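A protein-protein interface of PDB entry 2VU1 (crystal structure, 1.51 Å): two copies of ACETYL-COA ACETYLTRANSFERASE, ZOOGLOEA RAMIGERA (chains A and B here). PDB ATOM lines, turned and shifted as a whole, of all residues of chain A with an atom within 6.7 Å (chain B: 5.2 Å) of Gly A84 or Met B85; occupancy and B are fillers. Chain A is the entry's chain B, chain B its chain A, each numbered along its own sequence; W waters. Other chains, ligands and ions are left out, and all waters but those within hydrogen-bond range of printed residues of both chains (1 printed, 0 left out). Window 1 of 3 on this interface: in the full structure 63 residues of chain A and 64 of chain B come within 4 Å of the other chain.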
ATOM      1  N   VAL A  52      14.562 -27.884 -21.024  1.00  0.00           N
ATOM      2  CA  VAL A  52      14.301 -26.478 -21.245  1.00  0.00           C
ATOM      3  C   VAL A  52      12.949 -26.308 -21.969  1.00  0.00           C
ATOM      4  O   VAL A  52      12.666 -27.022 -22.947  1.00  0.00           O
ATOM      5  CB  VAL A  52      15.459 -25.919 -22.082  1.00  0.00           C
ATOM      6  CG1 VAL A  52      15.141 -24.459 -22.552  1.00  0.00           C
ATOM      7  CG2 VAL A  52      16.785 -26.102 -21.342  1.00  0.00           C
ATOM      8  N   ILE A  53      12.128 -25.400 -21.477  1.00  0.00           N
ATOM      9  CA  ILE A  53      10.789 -25.262 -22.016  1.00  0.00           C
ATOM     10  C   ILE A  53      10.577 -23.822 -22.275  1.00  0.00           C
ATOM     11  O   ILE A  53      10.657 -22.983 -21.339  1.00  0.00           O
ATOM     12  CB  ILE A  53       9.727 -25.686 -21.064  1.00  0.00           C
ATOM     13  CG1 ILE A  53       9.993 -27.127 -20.595  1.00  0.00           C
ATOM     14  CG2 ILE A  53       8.295 -25.403 -21.719  1.00  0.00           C
ATOM     15  CD1 ILE A  53       9.028 -27.566 -19.408  1.00  0.00           C
ATOM     16  N   LEU A  54      10.467 -23.473 -23.551  1.00  0.00           N
ATOM     17  CA  LEU A  54      10.420 -22.084 -23.916  1.00  0.00           C
ATOM     18  C   LEU A  54       9.164 -21.686 -24.713  1.00  0.00           C
ATOM     19  O   LEU A  54       8.837 -22.282 -25.695  1.00  0.00           O
ATOM     20  CB  LEU A  54      11.666 -21.703 -24.622  1.00  0.00           C
ATOM     21  CG  LEU A  54      12.903 -21.617 -23.724  1.00  0.00           C
ATOM     22  CD1 LEU A  54      14.072 -21.416 -24.640  1.00  0.00           C
ATOM     23  CD2 LEU A  54      12.756 -20.537 -22.734  1.00  0.00           C
ATOM     24  N   GLY A  55       8.356 -20.779 -24.233  1.00  0.00           N
ATOM     25  CA  GLY A  55       7.270 -20.290 -25.039  1.00  0.00           C
ATOM     26  C   GLY A  55       7.786 -19.475 -26.180  1.00  0.00           C
ATOM     27  O   GLY A  55       8.788 -18.733 -25.993  1.00  0.00           O
ATOM     28  N   GLN A  56       7.119 -19.588 -27.300  1.00  0.00           N
ATOM     29  CA  GLN A  56       7.562 -18.892 -28.505  1.00  0.00           C
ATOM     30  C   GLN A  56       6.433 -18.944 -29.507  1.00  0.00           C
ATOM     31  O   GLN A  56       5.972 -20.003 -29.860  1.00  0.00           O
ATOM     32  CB  GLN A  56       8.844 -19.519 -29.101  1.00  0.00           C
ATOM     33  CG  GLN A  56       9.367 -18.680 -30.260  1.00  0.00           C
ATOM     34  CD  GLN A  56      10.671 -19.162 -30.838  1.00  0.00           C
ATOM     35  OE1 GLN A  56      11.340 -18.463 -31.702  1.00  0.00           O
ATOM     36  NE2 GLN A  56      11.013 -20.405 -30.482  1.00  0.00           N
ATOM     37  N   ASN A  65      13.019 -26.640 -33.828  1.00  0.00           N
ATOM     38  CA  ASN A  65      12.805 -26.516 -32.329  1.00  0.00           C
ATOM     39  C   ASN A  65      13.774 -25.545 -31.660  1.00  0.00           C
ATOM     40  O   ASN A  65      14.802 -25.882 -31.140  1.00  0.00           O
ATOM     41  CB  ASN A  65      12.866 -27.877 -31.723  1.00  0.00           C
ATOM     42  CG  ASN A  65      12.669 -27.926 -30.270  1.00  0.00           C
ATOM     43  OD1 ASN A  65      12.046 -27.087 -29.592  1.00  0.00           O
ATOM     44  ND2 ASN A  65      13.059 -29.051 -29.793  1.00  0.00           N
ATOM     45  N   PRO A  66      13.549 -24.242 -31.902  1.00  0.00           N
ATOM     46  CA  PRO A  66      14.473 -23.205 -31.405  1.00  0.00           C
ATOM     47  C   PRO A  66      14.758 -23.308 -29.909  1.00  0.00           C
ATOM     48  O   PRO A  66      15.820 -22.890 -29.487  1.00  0.00           O
ATOM     49  CB  PRO A  66      13.769 -21.896 -31.778  1.00  0.00           C
ATOM     50  CG  PRO A  66      12.944 -22.289 -32.959  1.00  0.00           C
ATOM     51  CD  PRO A  66      12.473 -23.671 -32.754  1.00  0.00           C
ATOM     52  N   ALA A  67      13.879 -23.898 -29.096  1.00  0.00           N
ATOM     53  CA  ALA A  67      14.175 -24.169 -27.704  1.00  0.00           C
ATOM     54  C   ALA A  67      15.439 -25.012 -27.556  1.00  0.00           C
ATOM     55  O   ALA A  67      16.231 -24.839 -26.654  1.00  0.00           O
ATOM     56  CB  ALA A  67      12.964 -24.883 -26.932  1.00  0.00           C
ATOM     57  N   ARG A  68      15.494 -26.047 -28.347  1.00  0.00           N
ATOM     58  CA  ARG A  68      16.642 -26.995 -28.297  1.00  0.00           C
ATOM     59  C   ARG A  68      17.871 -26.215 -28.752  1.00  0.00           C
ATOM     60  O   ARG A  68      18.959 -26.478 -28.242  1.00  0.00           O
ATOM     61  CB  ARG A  68      16.443 -28.146 -29.244  1.00  0.00           C
ATOM     62  CG  ARG A  68      17.643 -29.133 -29.296  1.00  0.00           C
ATOM     63  CD  ARG A  68      17.835 -29.884 -27.990  1.00  0.00           C
ATOM     64  NE  ARG A  68      18.607 -31.103 -28.352  1.00  0.00           N
ATOM     65  CZ  ARG A  68      18.947 -32.040 -27.469  1.00  0.00           C
ATOM     66  NH1 ARG A  68      18.722 -31.799 -26.231  1.00  0.00           N
ATOM     67  NH2 ARG A  68      19.532 -33.163 -27.831  1.00  0.00           N
ATOM     68  N   ALA A  82      14.306 -30.459 -24.699  1.00  0.00           N
ATOM     69  CA  ALA A  82      13.847 -29.070 -24.796  1.00  0.00           C
ATOM     70  C   ALA A  82      12.698 -29.076 -25.792  1.00  0.00           C
ATOM     71  O   ALA A  82      12.669 -29.909 -26.731  1.00  0.00           O
ATOM     72  CB  ALA A  82      14.920 -28.201 -25.360  1.00  0.00           C
ATOM     73  N   TRP A  83      11.783 -28.125 -25.578  1.00  0.00           N
ATOM     74  CA  TRP A  83      10.624 -27.970 -26.436  1.00  0.00           C
ATOM     75  C   TRP A  83      10.046 -26.621 -26.307  1.00  0.00           C
ATOM     76  O   TRP A  83      10.313 -25.879 -25.332  1.00  0.00           O
ATOM     77  CB  TRP A  83       9.618 -29.059 -26.125  1.00  0.00           C
ATOM     78  CG  TRP A  83       9.180 -29.268 -24.660  1.00  0.00           C
ATOM     79  CD1 TRP A  83       9.867 -29.928 -23.670  1.00  0.00           C
ATOM     80  CD2 TRP A  83       7.954 -28.852 -24.070  1.00  0.00           C
ATOM     81  NE1 TRP A  83       9.164 -29.901 -22.505  1.00  0.00           N
ATOM     82  CE2 TRP A  83       7.937 -29.336 -22.743  1.00  0.00           C
ATOM     83  CE3 TRP A  83       6.817 -28.225 -24.549  1.00  0.00           C
ATOM     84  CZ2 TRP A  83       6.897 -29.037 -21.873  1.00  0.00           C
ATOM     85  CZ3 TRP A  83       5.816 -27.936 -23.715  1.00  0.00           C
ATOM     86  CH2 TRP A  83       5.804 -28.433 -22.400  1.00  0.00           C
ATOM     87  N   GLY A  84       9.229 -26.263 -27.300  1.00  0.00           N
ATOM     88  CA  GLY A  84       8.625 -24.964 -27.359  1.00  0.00           C
ATOM     89  C   GLY A  84       7.116 -25.149 -27.181  1.00  0.00           C
ATOM     90  O   GLY A  84       6.505 -26.235 -27.352  1.00  0.00           O
ATOM     91  N   MET A  85       6.482 -24.056 -26.795  1.00  0.00           N
ATOM     92  CA  MET A  85       5.052 -24.057 -26.744  1.00  0.00           C
ATOM     93  C   MET A  85       4.443 -22.716 -26.987  1.00  0.00           C
ATOM     94  O   MET A  85       5.137 -21.698 -26.995  1.00  0.00           O
ATOM     95  CB  MET A  85       4.624 -24.706 -25.444  1.00  0.00           C
ATOM     96  CG  MET A  85       5.137 -24.078 -24.126  1.00  0.00           C
ATOM     97  SD  MET A  85       4.454 -22.532 -23.635  1.00  0.00           S
ATOM     98  CE  MET A  85       2.683 -22.846 -23.555  1.00  0.00           C
ATOM     99  N   ASN A  86       3.131 -22.718 -27.183  1.00  0.00           N
ATOM    100  CA  ASN A  86       2.465 -21.530 -27.635  1.00  0.00           C
ATOM    101  C   ASN A  86       1.103 -21.503 -27.002  1.00  0.00           C
ATOM    102  O   ASN A  86       0.230 -22.224 -27.452  1.00  0.00           O
ATOM    103  CB  ASN A  86       2.400 -21.509 -29.168  1.00  0.00           C
ATOM    104  CG  ASN A  86       1.672 -20.298 -29.725  1.00  0.00           C
ATOM    105  OD1 ASN A  86       1.335 -19.389 -28.974  1.00  0.00           O
ATOM    106  ND2 ASN A  86       1.425 -20.293 -30.997  1.00  0.00           N
ATOM    107  N   ILE B  53      -4.606 -29.720 -26.053  1.00  0.00           N
ATOM    108  CA  ILE B  53      -3.149 -29.610 -26.159  1.00  0.00           C
ATOM    109  C   ILE B  53      -2.768 -30.326 -27.409  1.00  0.00           C
ATOM    110  O   ILE B  53      -2.880 -31.530 -27.507  1.00  0.00           O
ATOM    111  CB  ILE B  53      -2.433 -30.241 -24.991  1.00  0.00           C
ATOM    112  CG1 ILE B  53      -2.999 -29.688 -23.693  1.00  0.00           C
ATOM    113  CG2 ILE B  53      -0.856 -30.017 -25.201  1.00  0.00           C
ATOM    114  CD1 ILE B  53      -2.352 -30.371 -22.406  1.00  0.00           C
ATOM    115  N   LEU B  54      -2.336 -29.564 -28.393  1.00  0.00           N
ATOM    116  CA  LEU B  54      -2.019 -30.129 -29.683  1.00  0.00           C
ATOM    117  C   LEU B  54      -0.568 -29.825 -30.171  1.00  0.00           C
ATOM    118  O   LEU B  54      -0.146 -28.686 -30.326  1.00  0.00           O
ATOM    119  CB  LEU B  54      -3.006 -29.617 -30.702  1.00  0.00           C
ATOM    120  CG  LEU B  54      -4.429 -30.232 -30.526  1.00  0.00           C
ATOM    121  CD1 LEU B  54      -5.342 -29.406 -31.399  1.00  0.00           C
ATOM    122  CD2 LEU B  54      -4.541 -31.663 -30.860  1.00  0.00           C
ATOM    123  N   GLY B  55       0.217 -30.861 -30.422  1.00  0.00           N
ATOM    124  CA  GLY B  55       1.535 -30.704 -30.917  1.00  0.00           C
ATOM    125  C   GLY B  55       1.374 -30.270 -32.338  1.00  0.00           C
ATOM    126  O   GLY B  55       0.425 -30.717 -33.006  1.00  0.00           O
ATOM    127  N   GLN B  56       2.242 -29.395 -32.859  1.00  0.00           N
ATOM    128  CA  GLN B  56       2.211 -28.841 -34.224  1.00  0.00           C
ATOM    129  C   GLN B  56       3.529 -28.185 -34.421  1.00  0.00           C
ATOM    130  O   GLN B  56       3.948 -27.333 -33.679  1.00  0.00           O
ATOM    131  CB  GLN B  56       1.055 -27.860 -34.452  1.00  0.00           C
ATOM    132  CG  GLN B  56       0.985 -27.329 -35.840  1.00  0.00           C
ATOM    133  CD  GLN B  56      -0.211 -26.525 -36.097  1.00  0.00           C
ATOM    134  OE1 GLN B  56      -0.593 -26.263 -37.290  1.00  0.00           O
ATOM    135  NE2 GLN B  56      -0.786 -26.026 -35.019  1.00  0.00           N
ATOM    136  N   VAL B  57       4.223 -28.598 -35.486  1.00  0.00           N
ATOM    137  CA  VAL B  57       5.550 -28.109 -35.789  1.00  0.00           C
ATOM    138  C   VAL B  57       5.510 -26.996 -36.795  1.00  0.00           C
ATOM    139  O   VAL B  57       6.390 -26.158 -36.792  1.00  0.00           O
ATOM    140  CB  VAL B  57       6.405 -29.327 -36.251  1.00  0.00           C
ATOM    141  CG1 VAL B  57       7.817 -28.881 -36.678  1.00  0.00           C
ATOM    142  CG2 VAL B  57       6.456 -30.402 -35.147  1.00  0.00           C
ATOM    143  N   TRP B  83      -3.648 -24.844 -26.320  1.00  0.00           N
ATOM    144  CA  TRP B  83      -2.301 -24.375 -26.654  1.00  0.00           C
ATOM    145  C   TRP B  83      -1.609 -25.444 -27.455  1.00  0.00           C
ATOM    146  O   TRP B  83      -2.054 -26.615 -27.538  1.00  0.00           O
ATOM    147  CB  TRP B  83      -1.576 -24.081 -25.376  1.00  0.00           C
ATOM    148  CG  TRP B  83      -1.500 -25.154 -24.304  1.00  0.00           C
ATOM    149  CD1 TRP B  83      -2.495 -25.487 -23.352  1.00  0.00           C
ATOM    150  CD2 TRP B  83      -0.391 -26.034 -23.973  1.00  0.00           C
ATOM    151  NE1 TRP B  83      -2.062 -26.444 -22.527  1.00  0.00           N
ATOM    152  CE2 TRP B  83      -0.760 -26.750 -22.818  1.00  0.00           C
ATOM    153  CE3 TRP B  83       0.883 -26.229 -24.497  1.00  0.00           C
ATOM    154  CZ2 TRP B  83       0.067 -27.722 -22.246  1.00  0.00           C
ATOM    155  CZ3 TRP B  83       1.702 -27.167 -23.927  1.00  0.00           C
ATOM    156  CH2 TRP B  83       1.321 -27.860 -22.778  1.00  0.00           C
ATOM    157  N   GLY B  84      -0.599 -24.983 -28.196  1.00  0.00           N
ATOM    158  CA  GLY B  84       0.223 -25.757 -29.060  1.00  0.00           C
ATOM    159  C   GLY B  84       1.585 -25.994 -28.450  1.00  0.00           C
ATOM    160  O   GLY B  84       2.050 -25.256 -27.623  1.00  0.00           O
ATOM    161  N   MET B  85       2.230 -27.044 -28.893  1.00  0.00           N
ATOM    162  CA  MET B  85       3.593 -27.285 -28.478  1.00  0.00           C
ATOM    163  C   MET B  85       4.352 -27.990 -29.581  1.00  0.00           C
ATOM    164  O   MET B  85       3.793 -28.521 -30.541  1.00  0.00           O
ATOM    165  CB  MET B  85       3.624 -28.019 -27.156  1.00  0.00           C
ATOM    166  CG  MET B  85       2.893 -29.343 -26.972  1.00  0.00           C
ATOM    167  SD  MET B  85       3.616 -30.726 -27.755  1.00  0.00           S
ATOM    168  CE  MET B  85       5.265 -30.818 -27.140  1.00  0.00           C
ATOM    169  N   ASN B  86       5.657 -28.014 -29.370  1.00  0.00           N
ATOM    170  CA  ASN B  86       6.579 -28.534 -30.374  1.00  0.00           C
ATOM    171  C   ASN B  86       7.761 -29.165 -29.701  1.00  0.00           C
ATOM    172  O   ASN B  86       8.593 -28.491 -29.139  1.00  0.00           O
ATOM    173  CB  ASN B  86       7.018 -27.414 -31.356  1.00  0.00           C
ATOM    174  CG  ASN B  86       8.037 -27.849 -32.425  1.00  0.00           C
ATOM    175  OD1 ASN B  86       8.366 -29.002 -32.590  1.00  0.00           O
ATOM    176  ND2 ASN B  86       8.536 -26.875 -33.129  1.00  0.00           N
ATOM    177  N   GLN B  87       7.790 -30.484 -29.789  1.00  0.00           N
ATOM    178  CA  GLN B  87       9.011 -31.255 -29.573  1.00  0.00           C
ATOM    179  C   GLN B  87       9.143 -32.143 -30.837  1.00  0.00           C
ATOM    180  O   GLN B  87       9.337 -33.318 -30.778  1.00  0.00           O
ATOM    181  CB  GLN B  87       8.911 -32.026 -28.323  1.00  0.00           C
ATOM    182  CG  GLN B  87      10.205 -32.559 -27.788  1.00  0.00           C
ATOM    183  CD  GLN B  87      10.058 -33.429 -26.557  1.00  0.00           C
ATOM    184  OE1 GLN B  87       8.964 -33.649 -25.958  1.00  0.00           O
ATOM    185  NE2 GLN B  87      11.198 -34.050 -26.170  1.00  0.00           N
ATOM    186  N   SER B  91       6.055 -34.598 -30.787  1.00  0.00           N
ATOM    187  CA  SER B  91       5.103 -33.635 -30.237  1.00  0.00           C
ATOM    188  C   SER B  91       3.734 -34.248 -29.934  1.00  0.00           C
ATOM    189  O   SER B  91       3.164 -34.028 -28.867  1.00  0.00           O
ATOM    190  CB  SER B  91       4.825 -32.564 -31.241  1.00  0.00           C
ATOM    191  OG  SER B  91       5.916 -31.781 -31.512  1.00  0.00           O
ATOM    192  N   ARG B  94       4.150 -36.369 -26.876  1.00  0.00           N
ATOM    193  CA  ARG B  94       4.469 -35.562 -25.718  1.00  0.00           C
ATOM    194  C   ARG B  94       3.232 -34.821 -25.232  1.00  0.00           C
ATOM    195  O   ARG B  94       3.033 -34.715 -24.035  1.00  0.00           O
ATOM    196  CB  ARG B  94       5.613 -34.591 -26.067  1.00  0.00           C
ATOM    197  CG  ARG B  94       5.934 -33.715 -24.841  1.00  0.00           C
ATOM    198  CD  ARG B  94       6.540 -34.600 -23.706  1.00  0.00           C
ATOM    199  NE  ARG B  94       6.818 -33.873 -22.529  1.00  0.00           N
ATOM    200  CZ  ARG B  94       7.934 -33.261 -22.226  1.00  0.00           C
ATOM    201  NH1 ARG B  94       8.876 -33.046 -23.124  1.00  0.00           N
ATOM    202  NH2 ARG B  94       7.995 -32.744 -20.993  1.00  0.00           N
ATOM    203  N   ALA B  95       2.377 -34.361 -26.120  1.00  0.00           N
ATOM    204  CA  ALA B  95       1.136 -33.689 -25.741  1.00  0.00           C
ATOM    205  C   ALA B  95       0.271 -34.533 -24.823  1.00  0.00           C
ATOM    206  O   ALA B  95      -0.385 -34.052 -23.855  1.00  0.00           O
ATOM    207  CB  ALA B  95       0.370 -33.222 -26.969  1.00  0.00           C
ATOM    208  N   LEU B  98       1.784 -34.468 -21.506  1.00  0.00           N
ATOM    209  CA  LEU B  98       1.504 -33.145 -20.882  1.00  0.00           C
ATOM    210  C   LEU B  98       0.069 -33.087 -20.376  1.00  0.00           C
ATOM    211  O   LEU B  98      -0.222 -32.521 -19.314  1.00  0.00           O
ATOM    212  CB  LEU B  98       1.780 -32.081 -21.914  1.00  0.00           C
ATOM    213  CG  LEU B  98       3.275 -31.871 -22.083  1.00  0.00           C
ATOM    214  CD1 LEU B  98       3.525 -31.035 -23.377  1.00  0.00           C
ATOM    215  CD2 LEU B  98       3.894 -31.221 -20.850  1.00  0.00           C
HETATM  216  O   HOH W   1      10.443 -26.695 -35.304  1.00  0.00           O
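The backbone NH of Leu B54 sits at hydrogen-bond distance from the backbone carbonyl oxygen of Trp B83 (3.1 Å). The backbone carbonyl oxygen (O) of Met B85 sits at hydrogen-bond distance from the backbone NH (N) of Gln B56, at 2.9 Å. The backbone NH (N) of Gln B87 lies within hydrogen-bond range of the side-chain hydroxyl (OG) of Ser B91 (2.9 Å). The guanidinium group (NH1) of Arg B94 lies within hydrogen-bond range of the side-chain amide oxygen (OE1) of Gln B87 (2.9 Å). The backbone carbonyl oxygen (O) of Leu A54 lies within hydrogen-bond range of the backbone NH (N) of Met A85 (3.1 Å). The backbone carbonyl oxygen (O) of Met A85 sits at hydrogen-bond distance from the backbone NH (N) of Gln A56 (2.9 Å).
The backbone NH (N) of Asn A86 sits at hydrogen-bond distance from the backbone carbonyl oxygen (O) of Gly B84 (2.8 Å). N of Asn B86 lies within hydrogen-bond range of O of Gly A84, at 2.8 Å. The guanidinium group of Arg B94 lies close to the indole nitrogen of Trp A83, at 3.2 Å.
Water W1 lies within hydrogen-bond range of the side-chain amide nitrogen (ND2) of Asn B86 (2.9 Å) and the backbone NH (N) of Asn A65 (3.0 Å).
Trp A83 touches Met B85, and with the chains exchanged Met A85 touches Trp B83. Gly A84 touches Met B85, and with the chains exchanged Met A85 touches Gly B84. Gly A84 touches Asn B86, and with the chains exchanged Asn A86 touches Gly B84. Met A85 touches its own counterpart, Met B85. 8 positions are printed for both chains.
Gly A84 touches just these residues of chain B: Met B85 and Asn B86. Printed residues of chain A within 4 Å of Met B85: Trp A83, Gly A84 and Met A85. Of the printed residues of chain B, Met A85 touches Trp B83, Gly B84 and Met B85. Of the printed residues of chain A, Leu B98 touches Trp A83. Printed residues of chain A within 4 Å of Gln B87: Ala A82 and Trp A83. Of the printed residues of chain B, Asn A65 touches Asn B86 (3.8 Å). Printed residues of chain B within 4 Å of Ala A82: Gln B87. The nearest printed residue of chain A that does not touch Met B85 is Asn A86 (4.7 Å).
Asn B86 touches Asn A65 (O to OD1, 3.8 Å). CG of Gln B87 touches O of Ala A82, 3.8 Å away. Met B85 touches Trp A83 (CE to CE3, 3.98 Å). Trp A83 touches Asn B86. CB of Trp A83 touches CB of Gln B87, at 3.8 Å. CD1 of Leu B98 touches CH2 of Trp A83, at 3.6 Å. Trp B83 touches Met A85 (CE3 to CE, 3.9 Å). O of Gly B84 touches CA of Met A85 (3.3 Å). Met A85 touches Met B85 (CB to CB, 3.9 Å). Asn A86 touches Trp B83 (O to CB, 3.3 Å).
Printed residues of chain B that touch a printed residue of chain A: Trp B83, Gly B84, Met B85, Asn B86, Gln B87, Arg B94 and Leu B98. Hydrophobic or aromatic side chains of chain B within 4 Å of the printed part of chain A: Trp B83, Met B85 and Leu B98. Printed residues of chain A that touch a printed residue of chain B: Asn A65, Ala A82, Trp A83, Gly A84, Met A85 and Asn A86. Hydrophobic or aromatic side chains of chain A that line the printed part of chain B: Trp A83 and Met A85. Along chain A the printed residues that touch a printed residue of chain B span positions 65 to 86. Among the printed residues, no Asp or Glu carboxylate lies within 4 Å of a Lys or Arg side-chain nitrogen of the other chain.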
